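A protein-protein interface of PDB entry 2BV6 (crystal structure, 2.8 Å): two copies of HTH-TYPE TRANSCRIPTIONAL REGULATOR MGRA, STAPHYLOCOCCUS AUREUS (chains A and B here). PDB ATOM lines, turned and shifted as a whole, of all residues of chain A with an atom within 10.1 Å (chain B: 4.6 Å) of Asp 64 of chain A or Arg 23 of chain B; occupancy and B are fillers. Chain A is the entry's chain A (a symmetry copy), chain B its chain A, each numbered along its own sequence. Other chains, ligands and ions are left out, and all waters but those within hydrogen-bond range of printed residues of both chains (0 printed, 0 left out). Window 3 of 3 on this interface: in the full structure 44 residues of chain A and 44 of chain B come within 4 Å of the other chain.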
ATOM      1  N   VAL A  54       2.841 -23.792  -6.426  1.00  0.00           N
ATOM      2  CA  VAL A  54       2.238 -22.659  -5.758  1.00  0.00           C
ATOM      3  C   VAL A  54       2.869 -22.388  -4.406  1.00  0.00           C
ATOM      4  O   VAL A  54       2.997 -21.236  -4.000  1.00  0.00           O
ATOM      5  CB  VAL A  54       0.736 -22.861  -5.571  1.00  0.00           C
ATOM      6  CG1 VAL A  54       0.194 -21.836  -4.614  1.00  0.00           C
ATOM      7  CG2 VAL A  54       0.037 -22.718  -6.903  1.00  0.00           C
ATOM      8  N   LYS A  55       3.276 -23.441  -3.710  1.00  0.00           N
ATOM      9  CA  LYS A  55       3.872 -23.284  -2.393  1.00  0.00           C
ATOM     10  C   LYS A  55       5.056 -22.340  -2.402  1.00  0.00           C
ATOM     11  O   LYS A  55       5.350 -21.718  -1.394  1.00  0.00           O
ATOM     12  CB  LYS A  55       4.280 -24.642  -1.818  1.00  0.00           C
ATOM     13  CG  LYS A  55       3.082 -25.510  -1.408  1.00  0.00           C
ATOM     14  CD  LYS A  55       3.492 -26.830  -0.746  1.00  0.00           C
ATOM     15  CE  LYS A  55       4.312 -27.729  -1.682  1.00  0.00           C
ATOM     16  NZ  LYS A  55       4.646 -29.059  -1.080  1.00  0.00           N
ATOM     17  N   VAL A  57       5.286 -19.593  -4.278  1.00  0.00           N
ATOM     18  CA  VAL A  57       4.772 -18.243  -4.307  1.00  0.00           C
ATOM     19  C   VAL A  57       4.397 -17.879  -2.887  1.00  0.00           C
ATOM     20  O   VAL A  57       4.760 -16.824  -2.398  1.00  0.00           O
ATOM     21  CB  VAL A  57       3.541 -18.132  -5.194  1.00  0.00           C
ATOM     22  CG1 VAL A  57       2.860 -16.794  -4.975  1.00  0.00           C
ATOM     23  CG2 VAL A  57       3.953 -18.266  -6.632  1.00  0.00           C
ATOM     24  N   VAL A  58       3.671 -18.762  -2.217  1.00  0.00           N
ATOM     25  CA  VAL A  58       3.277 -18.497  -0.839  1.00  0.00           C
ATOM     26  C   VAL A  58       4.501 -18.247   0.029  1.00  0.00           C
ATOM     27  O   VAL A  58       4.455 -17.438   0.949  1.00  0.00           O
ATOM     28  CB  VAL A  58       2.495 -19.673  -0.235  1.00  0.00           C
ATOM     29  CG1 VAL A  58       2.189 -19.395   1.213  1.00  0.00           C
ATOM     30  CG2 VAL A  58       1.213 -19.889  -1.010  1.00  0.00           C
ATOM     31  N   THR A  59       5.597 -18.937  -0.259  1.00  0.00           N
ATOM     32  CA  THR A  59       6.804 -18.759   0.531  1.00  0.00           C
ATOM     33  C   THR A  59       7.507 -17.435   0.291  1.00  0.00           C
ATOM     34  O   THR A  59       7.811 -16.729   1.237  1.00  0.00           O
ATOM     35  CB  THR A  59       7.825 -19.887   0.282  1.00  0.00           C
ATOM     36  OG1 THR A  59       7.466 -21.043   1.051  1.00  0.00           O
ATOM     37  CG2 THR A  59       9.212 -19.439   0.682  1.00  0.00           C
ATOM     38  N   GLU A  60       7.757 -17.097  -0.969  1.00  0.00           N
ATOM     39  CA  GLU A  60       8.466 -15.871  -1.302  1.00  0.00           C
ATOM     40  C   GLU A  60       7.710 -14.574  -1.058  1.00  0.00           C
ATOM     41  O   GLU A  60       8.278 -13.488  -1.147  1.00  0.00           O
ATOM     42  CB  GLU A  60       8.914 -15.929  -2.754  1.00  0.00           C
ATOM     43  CG  GLU A  60       9.648 -17.208  -3.089  1.00  0.00           C
ATOM     44  CD  GLU A  60      10.858 -17.444  -2.206  1.00  0.00           C
ATOM     45  OE1 GLU A  60      11.868 -16.729  -2.371  1.00  0.00           O
ATOM     46  OE2 GLU A  60      10.800 -18.343  -1.339  1.00  0.00           O
ATOM     47  N   LEU A  61       6.427 -14.676  -0.767  1.00  0.00           N
ATOM     48  CA  LEU A  61       5.640 -13.487  -0.512  1.00  0.00           C
ATOM     49  C   LEU A  61       4.963 -13.640   0.829  1.00  0.00           C
ATOM     50  O   LEU A  61       4.838 -14.747   1.342  1.00  0.00           O
ATOM     51  CB  LEU A  61       4.599 -13.284  -1.612  1.00  0.00           C
ATOM     52  CG  LEU A  61       5.109 -12.643  -2.914  1.00  0.00           C
ATOM     53  CD1 LEU A  61       6.275 -13.413  -3.464  1.00  0.00           C
ATOM     54  CD2 LEU A  61       3.992 -12.581  -3.933  1.00  0.00           C
ATOM     55  N   ALA A  62       4.545 -12.526   1.411  1.00  0.00           N
ATOM     56  CA  ALA A  62       3.878 -12.576   2.704  1.00  0.00           C
ATOM     57  C   ALA A  62       2.424 -12.988   2.482  1.00  0.00           C
ATOM     58  O   ALA A  62       1.486 -12.228   2.762  1.00  0.00           O
ATOM     59  CB  ALA A  62       3.955 -11.214   3.387  1.00  0.00           C
ATOM     60  N   LEU A  63       2.246 -14.201   1.968  1.00  0.00           N
ATOM     61  CA  LEU A  63       0.912 -14.696   1.697  1.00  0.00           C
ATOM     62  C   LEU A  63       0.330 -15.517   2.836  1.00  0.00           C
ATOM     63  O   LEU A  63       0.993 -16.385   3.414  1.00  0.00           O
ATOM     64  CB  LEU A  63       0.891 -15.515   0.401  1.00  0.00           C
ATOM     65  CG  LEU A  63       1.216 -14.790  -0.911  1.00  0.00           C
ATOM     66  CD1 LEU A  63       0.734 -15.645  -2.067  1.00  0.00           C
ATOM     67  CD2 LEU A  63       0.538 -13.433  -0.967  1.00  0.00           C
ATOM     68  N   ASP A  64      -0.929 -15.213   3.142  1.00  0.00           N
ATOM     69  CA  ASP A  64      -1.688 -15.873   4.193  1.00  0.00           C
ATOM     70  C   ASP A  64      -2.528 -16.959   3.548  1.00  0.00           C
ATOM     71  O   ASP A  64      -2.341 -17.297   2.376  1.00  0.00           O
ATOM     72  CB  ASP A  64      -2.611 -14.863   4.860  1.00  0.00           C
ATOM     73  CG  ASP A  64      -1.931 -13.539   5.090  1.00  0.00           C
ATOM     74  OD1 ASP A  64      -1.240 -13.398   6.123  1.00  0.00           O
ATOM     75  OD2 ASP A  64      -2.071 -12.650   4.222  1.00  0.00           O
ATOM     76  N   THR A  65      -3.462 -17.502   4.312  1.00  0.00           N
ATOM     77  CA  THR A  65      -4.320 -18.540   3.774  1.00  0.00           C
ATOM     78  C   THR A  65      -5.319 -17.888   2.831  1.00  0.00           C
ATOM     79  O   THR A  65      -5.666 -16.715   2.996  1.00  0.00           O
ATOM     80  CB  THR A  65      -5.079 -19.276   4.892  1.00  0.00           C
ATOM     81  OG1 THR A  65      -4.137 -19.819   5.828  1.00  0.00           O
ATOM     82  CG2 THR A  65      -5.923 -20.409   4.310  1.00  0.00           C
ATOM     83  N   GLY A  66      -5.756 -18.650   1.833  1.00  0.00           N
ATOM     84  CA  GLY A  66      -6.727 -18.157   0.877  1.00  0.00           C
ATOM     85  C   GLY A  66      -6.505 -16.750   0.349  1.00  0.00           C
ATOM     86  O   GLY A  66      -7.466 -16.055   0.009  1.00  0.00           O
ATOM     87  N   THR A  67      -5.253 -16.310   0.304  1.00  0.00           N
ATOM     88  CA  THR A  67      -4.945 -14.992  -0.240  1.00  0.00           C
ATOM     89  C   THR A  67      -4.187 -15.295  -1.529  1.00  0.00           C
ATOM     90  O   THR A  67      -4.227 -14.535  -2.497  1.00  0.00           O
ATOM     91  CB  THR A  67      -4.059 -14.166   0.717  1.00  0.00           C
ATOM     92  OG1 THR A  67      -2.803 -14.824   0.902  1.00  0.00           O
ATOM     93  CG2 THR A  67      -4.735 -14.019   2.064  1.00  0.00           C
ATOM     94  N   VAL A  68      -3.531 -16.449  -1.523  1.00  0.00           N
ATOM     95  CA  VAL A  68      -2.747 -16.948  -2.645  1.00  0.00           C
ATOM     96  C   VAL A  68      -3.669 -17.373  -3.776  1.00  0.00           C
ATOM     97  O   VAL A  68      -3.580 -16.876  -4.896  1.00  0.00           O
ATOM     98  CB  VAL A  68      -1.944 -18.186  -2.222  1.00  0.00           C
ATOM     99  CG1 VAL A  68      -0.858 -18.493  -3.248  1.00  0.00           C
ATOM    100  CG2 VAL A  68      -1.379 -17.975  -0.821  1.00  0.00           C
ATOM    101  N   SER A  69      -4.550 -18.312  -3.457  1.00  0.00           N
ATOM    102  CA  SER A  69      -5.500 -18.859  -4.413  1.00  0.00           C
ATOM    103  C   SER A  69      -6.180 -17.760  -5.213  1.00  0.00           C
ATOM    104  O   SER A  69      -6.239 -17.820  -6.443  1.00  0.00           O
ATOM    105  CB  SER A  69      -6.547 -19.680  -3.673  1.00  0.00           C
ATOM    106  OG  SER A  69      -6.027 -20.122  -2.433  1.00  0.00           O
ATOM    107  N   PRO A  70      -6.721 -16.745  -4.519  1.00  0.00           N
ATOM    108  CA  PRO A  70      -7.393 -15.639  -5.199  1.00  0.00           C
ATOM    109  C   PRO A  70      -6.435 -14.925  -6.131  1.00  0.00           C
ATOM    110  O   PRO A  70      -6.706 -14.806  -7.326  1.00  0.00           O
ATOM    111  CB  PRO A  70      -7.841 -14.753  -4.046  1.00  0.00           C
ATOM    112  CG  PRO A  70      -8.122 -15.750  -2.967  1.00  0.00           C
ATOM    113  CD  PRO A  70      -6.905 -16.637  -3.062  1.00  0.00           C
ATOM    114  N   LEU A  71      -5.314 -14.453  -5.589  1.00  0.00           N
ATOM    115  CA  LEU A  71      -4.330 -13.751  -6.406  1.00  0.00           C
ATOM    116  C   LEU A  71      -4.041 -14.509  -7.701  1.00  0.00           C
ATOM    117  O   LEU A  71      -4.141 -13.942  -8.793  1.00  0.00           O
ATOM    118  CB  LEU A  71      -3.033 -13.542  -5.620  1.00  0.00           C
ATOM    119  CG  LEU A  71      -1.752 -13.199  -6.395  1.00  0.00           C
ATOM    120  CD1 LEU A  71      -1.907 -11.939  -7.213  1.00  0.00           C
ATOM    121  CD2 LEU A  71      -0.629 -13.022  -5.410  1.00  0.00           C
ATOM    122  N   LEU A  72      -3.704 -15.792  -7.582  1.00  0.00           N
ATOM    123  CA  LEU A  72      -3.400 -16.600  -8.757  1.00  0.00           C
ATOM    124  C   LEU A  72      -4.601 -16.794  -9.672  1.00  0.00           C
ATOM    125  O   LEU A  72      -4.451 -16.864 -10.888  1.00  0.00           O
ATOM    126  CB  LEU A  72      -2.829 -17.951  -8.340  1.00  0.00           C
ATOM    127  CG  LEU A  72      -1.521 -17.840  -7.557  1.00  0.00           C
ATOM    128  CD1 LEU A  72      -1.027 -19.237  -7.183  1.00  0.00           C
ATOM    129  CD2 LEU A  72      -0.492 -17.072  -8.379  1.00  0.00           C
ATOM    130  N   VAL A 136      14.518  -7.338   9.368  1.00  0.00           N
ATOM    131  CA  VAL A 136      13.185  -6.770   9.573  1.00  0.00           C
ATOM    132  C   VAL A 136      12.122  -7.823   9.276  1.00  0.00           C
ATOM    133  O   VAL A 136      11.143  -7.972  10.014  1.00  0.00           O
ATOM    134  CB  VAL A 136      12.937  -5.563   8.630  1.00  0.00           C
ATOM    135  CG1 VAL A 136      11.622  -4.891   8.983  1.00  0.00           C
ATOM    136  CG2 VAL A 136      14.095  -4.574   8.716  1.00  0.00           C
ATOM    137  N   ILE A 137      12.337  -8.550   8.185  1.00  0.00           N
ATOM    138  CA  ILE A 137      11.416  -9.576   7.738  1.00  0.00           C
ATOM    139  C   ILE A 137      11.153 -10.674   8.755  1.00  0.00           C
ATOM    140  O   ILE A 137      10.008 -10.893   9.145  1.00  0.00           O
ATOM    141  CB  ILE A 137      11.911 -10.184   6.424  1.00  0.00           C
ATOM    142  CG1 ILE A 137      11.961  -9.082   5.361  1.00  0.00           C
ATOM    143  CG2 ILE A 137      10.993 -11.300   5.988  1.00  0.00           C
ATOM    144  CD1 ILE A 137      12.370  -9.529   3.974  1.00  0.00           C
ATOM    145  N   HIS A 138      12.202 -11.357   9.197  1.00  0.00           N
ATOM    146  CA  HIS A 138      12.035 -12.437  10.168  1.00  0.00           C
ATOM    147  C   HIS A 138      11.930 -11.901  11.585  1.00  0.00           C
ATOM    148  O   HIS A 138      11.830 -12.674  12.537  1.00  0.00           O
ATOM    149  CB  HIS A 138      13.207 -13.407  10.083  1.00  0.00           C
ATOM    150  CG  HIS A 138      13.424 -13.959   8.713  1.00  0.00           C
ATOM    151  ND1 HIS A 138      12.531 -14.815   8.107  1.00  0.00           N
ATOM    152  CD2 HIS A 138      14.411 -13.741   7.810  1.00  0.00           C
ATOM    153  CE1 HIS A 138      12.957 -15.099   6.888  1.00  0.00           C
ATOM    154  NE2 HIS A 138      14.096 -14.460   6.684  1.00  0.00           N
ATOM    155  N   ALA A 139      11.946 -10.578  11.716  1.00  0.00           N
ATOM    156  CA  ALA A 139      11.860  -9.923  13.018  1.00  0.00           C
ATOM    157  C   ALA A 139      10.697 -10.413  13.885  1.00  0.00           C
ATOM    158  O   ALA A 139      10.603 -10.057  15.059  1.00  0.00           O
ATOM    159  CB  ALA A 139      11.764  -8.414  12.828  1.00  0.00           C
ATOM    160  N   PHE A 140       9.809 -11.226  13.320  1.00  0.00           N
ATOM    161  CA  PHE A 140       8.679 -11.730  14.090  1.00  0.00           C
ATOM    162  C   PHE A 140       8.438 -13.212  13.826  1.00  0.00           C
ATOM    163  O   PHE A 140       7.311 -13.665  14.125  1.00  0.00           O
ATOM    164  CB  PHE A 140       7.413 -10.931  13.761  1.00  0.00           C
ATOM    165  CG  PHE A 140       7.628  -9.437  13.705  1.00  0.00           C
ATOM    166  CD1 PHE A 140       8.158  -8.839  12.565  1.00  0.00           C
ATOM    167  CD2 PHE A 140       7.312  -8.630  14.794  1.00  0.00           C
ATOM    168  CE1 PHE A 140       8.367  -7.459  12.513  1.00  0.00           C
ATOM    169  CE2 PHE A 140       7.521  -7.250  14.748  1.00  0.00           C
ATOM    170  CZ  PHE A 140       8.047  -6.667  13.609  1.00  0.00           C
ATOM    171  N   ARG B  19       5.625  -5.293   4.208  1.00  0.00           N
ATOM    172  CA  ARG B  19       4.521  -6.230   4.335  1.00  0.00           C
ATOM    173  C   ARG B  19       4.505  -6.877   5.718  1.00  0.00           C
ATOM    174  O   ARG B  19       3.459  -6.987   6.362  1.00  0.00           O
ATOM    175  CB  ARG B  19       4.631  -7.294   3.244  1.00  0.00           C
ATOM    176  CG  ARG B  19       3.392  -8.154   3.072  1.00  0.00           C
ATOM    177  CD  ARG B  19       2.170  -7.344   2.683  1.00  0.00           C
ATOM    178  NE  ARG B  19       1.004  -8.212   2.538  1.00  0.00           N
ATOM    179  CZ  ARG B  19      -0.215  -7.786   2.224  1.00  0.00           C
ATOM    180  NH1 ARG B  19      -0.434  -6.491   2.020  1.00  0.00           N
ATOM    181  NH2 ARG B  19      -1.215  -8.655   2.114  1.00  0.00           N
ATOM    182  N   GLN B  20       5.680  -7.289   6.177  1.00  0.00           N
ATOM    183  CA  GLN B  20       5.808  -7.918   7.485  1.00  0.00           C
ATOM    184  C   GLN B  20       5.473  -6.963   8.617  1.00  0.00           C
ATOM    185  O   GLN B  20       4.605  -7.248   9.449  1.00  0.00           O
ATOM    186  CB  GLN B  20       7.223  -8.465   7.669  1.00  0.00           C
ATOM    187  CG  GLN B  20       7.447  -9.755   6.919  1.00  0.00           C
ATOM    188  CD  GLN B  20       6.352 -10.755   7.223  1.00  0.00           C
ATOM    189  OE1 GLN B  20       6.177 -11.171   8.371  1.00  0.00           O
ATOM    190  NE2 GLN B  20       5.595 -11.132   6.198  1.00  0.00           N
ATOM    191  N   VAL B  21       6.168  -5.828   8.641  1.00  0.00           N
ATOM    192  CA  VAL B  21       5.946  -4.827   9.672  1.00  0.00           C
ATOM    193  C   VAL B  21       4.470  -4.427   9.747  1.00  0.00           C
ATOM    194  O   VAL B  21       3.941  -4.183  10.836  1.00  0.00           O
ATOM    195  CB  VAL B  21       6.789  -3.571   9.406  1.00  0.00           C
ATOM    196  CG1 VAL B  21       6.633  -2.596  10.542  1.00  0.00           C
ATOM    197  CG2 VAL B  21       8.238  -3.955   9.231  1.00  0.00           C
ATOM    198  N   ASN B  22       3.797  -4.355   8.601  1.00  0.00           N
ATOM    199  CA  ASN B  22       2.393  -3.982   8.630  1.00  0.00           C
ATOM    200  C   ASN B  22       1.618  -5.126   9.240  1.00  0.00           C
ATOM    201  O   ASN B  22       0.791  -4.917  10.129  1.00  0.00           O
ATOM    202  CB  ASN B  22       1.862  -3.680   7.230  1.00  0.00           C
ATOM    203  CG  ASN B  22       0.381  -3.291   7.237  1.00  0.00           C
ATOM    204  OD1 ASN B  22      -0.099  -2.637   6.313  1.00  0.00           O
ATOM    205  ND2 ASN B  22      -0.347  -3.701   8.271  1.00  0.00           N
ATOM    206  N   ARG B  23       1.888  -6.334   8.754  1.00  0.00           N
ATOM    207  CA  ARG B  23       1.226  -7.529   9.261  1.00  0.00           C
ATOM    208  C   ARG B  23       1.232  -7.505  10.788  1.00  0.00           C
ATOM    209  O   ARG B  23       0.183  -7.539  11.436  1.00  0.00           O
ATOM    210  CB  ARG B  23       1.952  -8.784   8.759  1.00  0.00           C
ATOM    211  CG  ARG B  23       1.550 -10.077   9.483  1.00  0.00           C
ATOM    212  CD  ARG B  23       2.189 -11.323   8.869  1.00  0.00           C
ATOM    213  NE  ARG B  23       1.678 -11.601   7.525  1.00  0.00           N
ATOM    214  CZ  ARG B  23       2.018 -12.659   6.794  1.00  0.00           C
ATOM    215  NH1 ARG B  23       2.874 -13.557   7.270  1.00  0.00           N
ATOM    216  NH2 ARG B  23       1.501 -12.820   5.583  1.00  0.00           N
ATOM    217  N   TYR B  24       2.431  -7.433  11.352  1.00  0.00           N
ATOM    218  CA  TYR B  24       2.597  -7.406  12.791  1.00  0.00           C
ATOM    219  C   TYR B  24       1.647  -6.433  13.458  1.00  0.00           C
ATOM    220  O   TYR B  24       0.729  -6.830  14.180  1.00  0.00           O
ATOM    221  CB  TYR B  24       4.030  -7.022  13.139  1.00  0.00           C
ATOM    222  CG  TYR B  24       4.261  -6.858  14.615  1.00  0.00           C
ATOM    223  CD1 TYR B  24       3.946  -7.881  15.507  1.00  0.00           C
ATOM    224  CD2 TYR B  24       4.816  -5.690  15.122  1.00  0.00           C
ATOM    225  CE1 TYR B  24       4.180  -7.745  16.869  1.00  0.00           C
ATOM    226  CE2 TYR B  24       5.058  -5.542  16.484  1.00  0.00           C
ATOM    227  CZ  TYR B  24       4.739  -6.574  17.351  1.00  0.00           C
ATOM    228  OH  TYR B  24       4.990  -6.430  18.696  1.00  0.00           O
ATOM    229  N   TYR B  25       1.880  -5.151  13.204  1.00  0.00           N
ATOM    230  CA  TYR B  25       1.073  -4.088  13.779  1.00  0.00           C
ATOM    231  C   TYR B  25      -0.399  -4.200  13.498  1.00  0.00           C
ATOM    232  O   TYR B  25      -1.223  -3.863  14.343  1.00  0.00           O
ATOM    233  CB  TYR B  25       1.582  -2.736  13.303  1.00  0.00           C
ATOM    234  CG  TYR B  25       2.761  -2.281  14.100  1.00  0.00           C
ATOM    235  CD1 TYR B  25       3.865  -1.698  13.482  1.00  0.00           C
ATOM    236  CD2 TYR B  25       2.792  -2.474  15.476  1.00  0.00           C
ATOM    237  CE1 TYR B  25       4.981  -1.323  14.217  1.00  0.00           C
ATOM    238  CE2 TYR B  25       3.897  -2.109  16.222  1.00  0.00           C
ATOM    239  CZ  TYR B  25       4.990  -1.537  15.589  1.00  0.00           C
ATOM    240  OH  TYR B  25       6.097  -1.209  16.333  1.00  0.00           O
ATOM    241  N   SER B  26      -0.747  -4.674  12.314  1.00  0.00           N
ATOM    242  CA  SER B  26      -2.151  -4.790  11.998  1.00  0.00           C
ATOM    243  C   SER B  26      -2.835  -5.694  13.021  1.00  0.00           C
ATOM    244  O   SER B  26      -3.948  -5.406  13.469  1.00  0.00           O
ATOM    245  CB  SER B  26      -2.331  -5.333  10.591  1.00  0.00           C
ATOM    246  OG  SER B  26      -3.586  -4.912  10.091  1.00  0.00           O
ATOM    247  N   ASN B  27      -2.151  -6.770  13.408  1.00  0.00           N
ATOM    248  CA  ASN B  27      -2.689  -7.716  14.388  1.00  0.00           C
ATOM    249  C   ASN B  27      -2.511  -7.250  15.829  1.00  0.00           C
ATOM    250  O   ASN B  27      -3.472  -7.189  16.588  1.00  0.00           O
ATOM    251  CB  ASN B  27      -2.034  -9.094  14.239  1.00  0.00           C
ATOM    252  CG  ASN B  27      -2.258  -9.705  12.872  1.00  0.00           C
ATOM    253  OD1 ASN B  27      -3.306  -9.513  12.255  1.00  0.00           O
ATOM    254  ND2 ASN B  27      -1.278 -10.460  12.399  1.00  0.00           N
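Of the 23 printed residues of chain A, 6 touch a printed residue of chain B. Of the 9 printed residues of chain B, 5 touch a printed residue of chain A. Printed residues of chain B that touch a printed residue of chain A: Arg 19, Gln 20, Val 21, Arg 23 and Tyr 24.
Of chain B, only Arg 23 (2.9 Å) comes within 4 Å of Asp 64 of chain A. Of chain A, only Ala 62, Leu 63 and Asp 64 come within 4 Å of Arg 23 of chain B. Of the printed residues of chain A, Gln 20 of chain B touches Ala 62 (3.3 Å) and Ile 137 (3.6 Å). No residue of chain A comes within 4 Å of Asn 22 of chain B. Of the printed residues of chain A, Arg 19 of chain B touches Ala 62. Printed residues of chain B within 4 Å of Ile 137 of chain A: Gln 20. Printed residues of chain A within 4 Å of Val 21 of chain B: Val 136. Of the printed residues of chain B, Phe 140 of chain A touches Tyr 24 (3.1 Å). Printed residues of chain B within 4 Å of Leu 63 of chain A: Arg 23. Ala 139 of chain A touches none of the printed residues of chain B. Leu 71 of chain A touches none of the printed residues of chain B. The nearest printed residue of chain B that does not touch Asp 64 of chain A is Arg 19 of chain B (4.6 Å). The nearest residue of chain A that does not touch Arg 23 of chain B is Leu 61 of chain A (5.7 Å).
The side-chain amide nitrogen of Asn 27 of chain B sits at hydrogen-bond distance from the backbone carbonyl oxygen of Arg 23 of chain B (3.4 Å). O of Asp 64 of chain A is in hydrogen-bond range of OG1 of Thr 67 of chain A (2.9 Å).
Among the printed residues, merely in contact across the chains: Ala 62 of chain A with Arg 19 of chain B (3.1 Å), Ala 62 of chain A with Gln 20 of chain B (3.3 Å), Leu 63 of chain A with Arg 23 of chain B (3.9 Å), Val 136 of chain A with Val 21 of chain B (3.5 Å), Ile 137 of chain A with Gln 20 of chain B (3.6 Å) and Phe 140 of chain A with Tyr 24 of chain B (3.1 Å).
NH2 of Arg 23 of chain B lies within salt-bridge range of OD1 of Asp 64 of chain A. The backbone carbonyl oxygen of Ala 62 of chain A sits at hydrogen-bond distance from the guanidinium group of Arg 23 of chain B, at 2.9 Å.
No position is printed for both chains. Of the 8 pairs that touch across the chains among the printed residues, none has its exchanged pair printed and touching as well.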
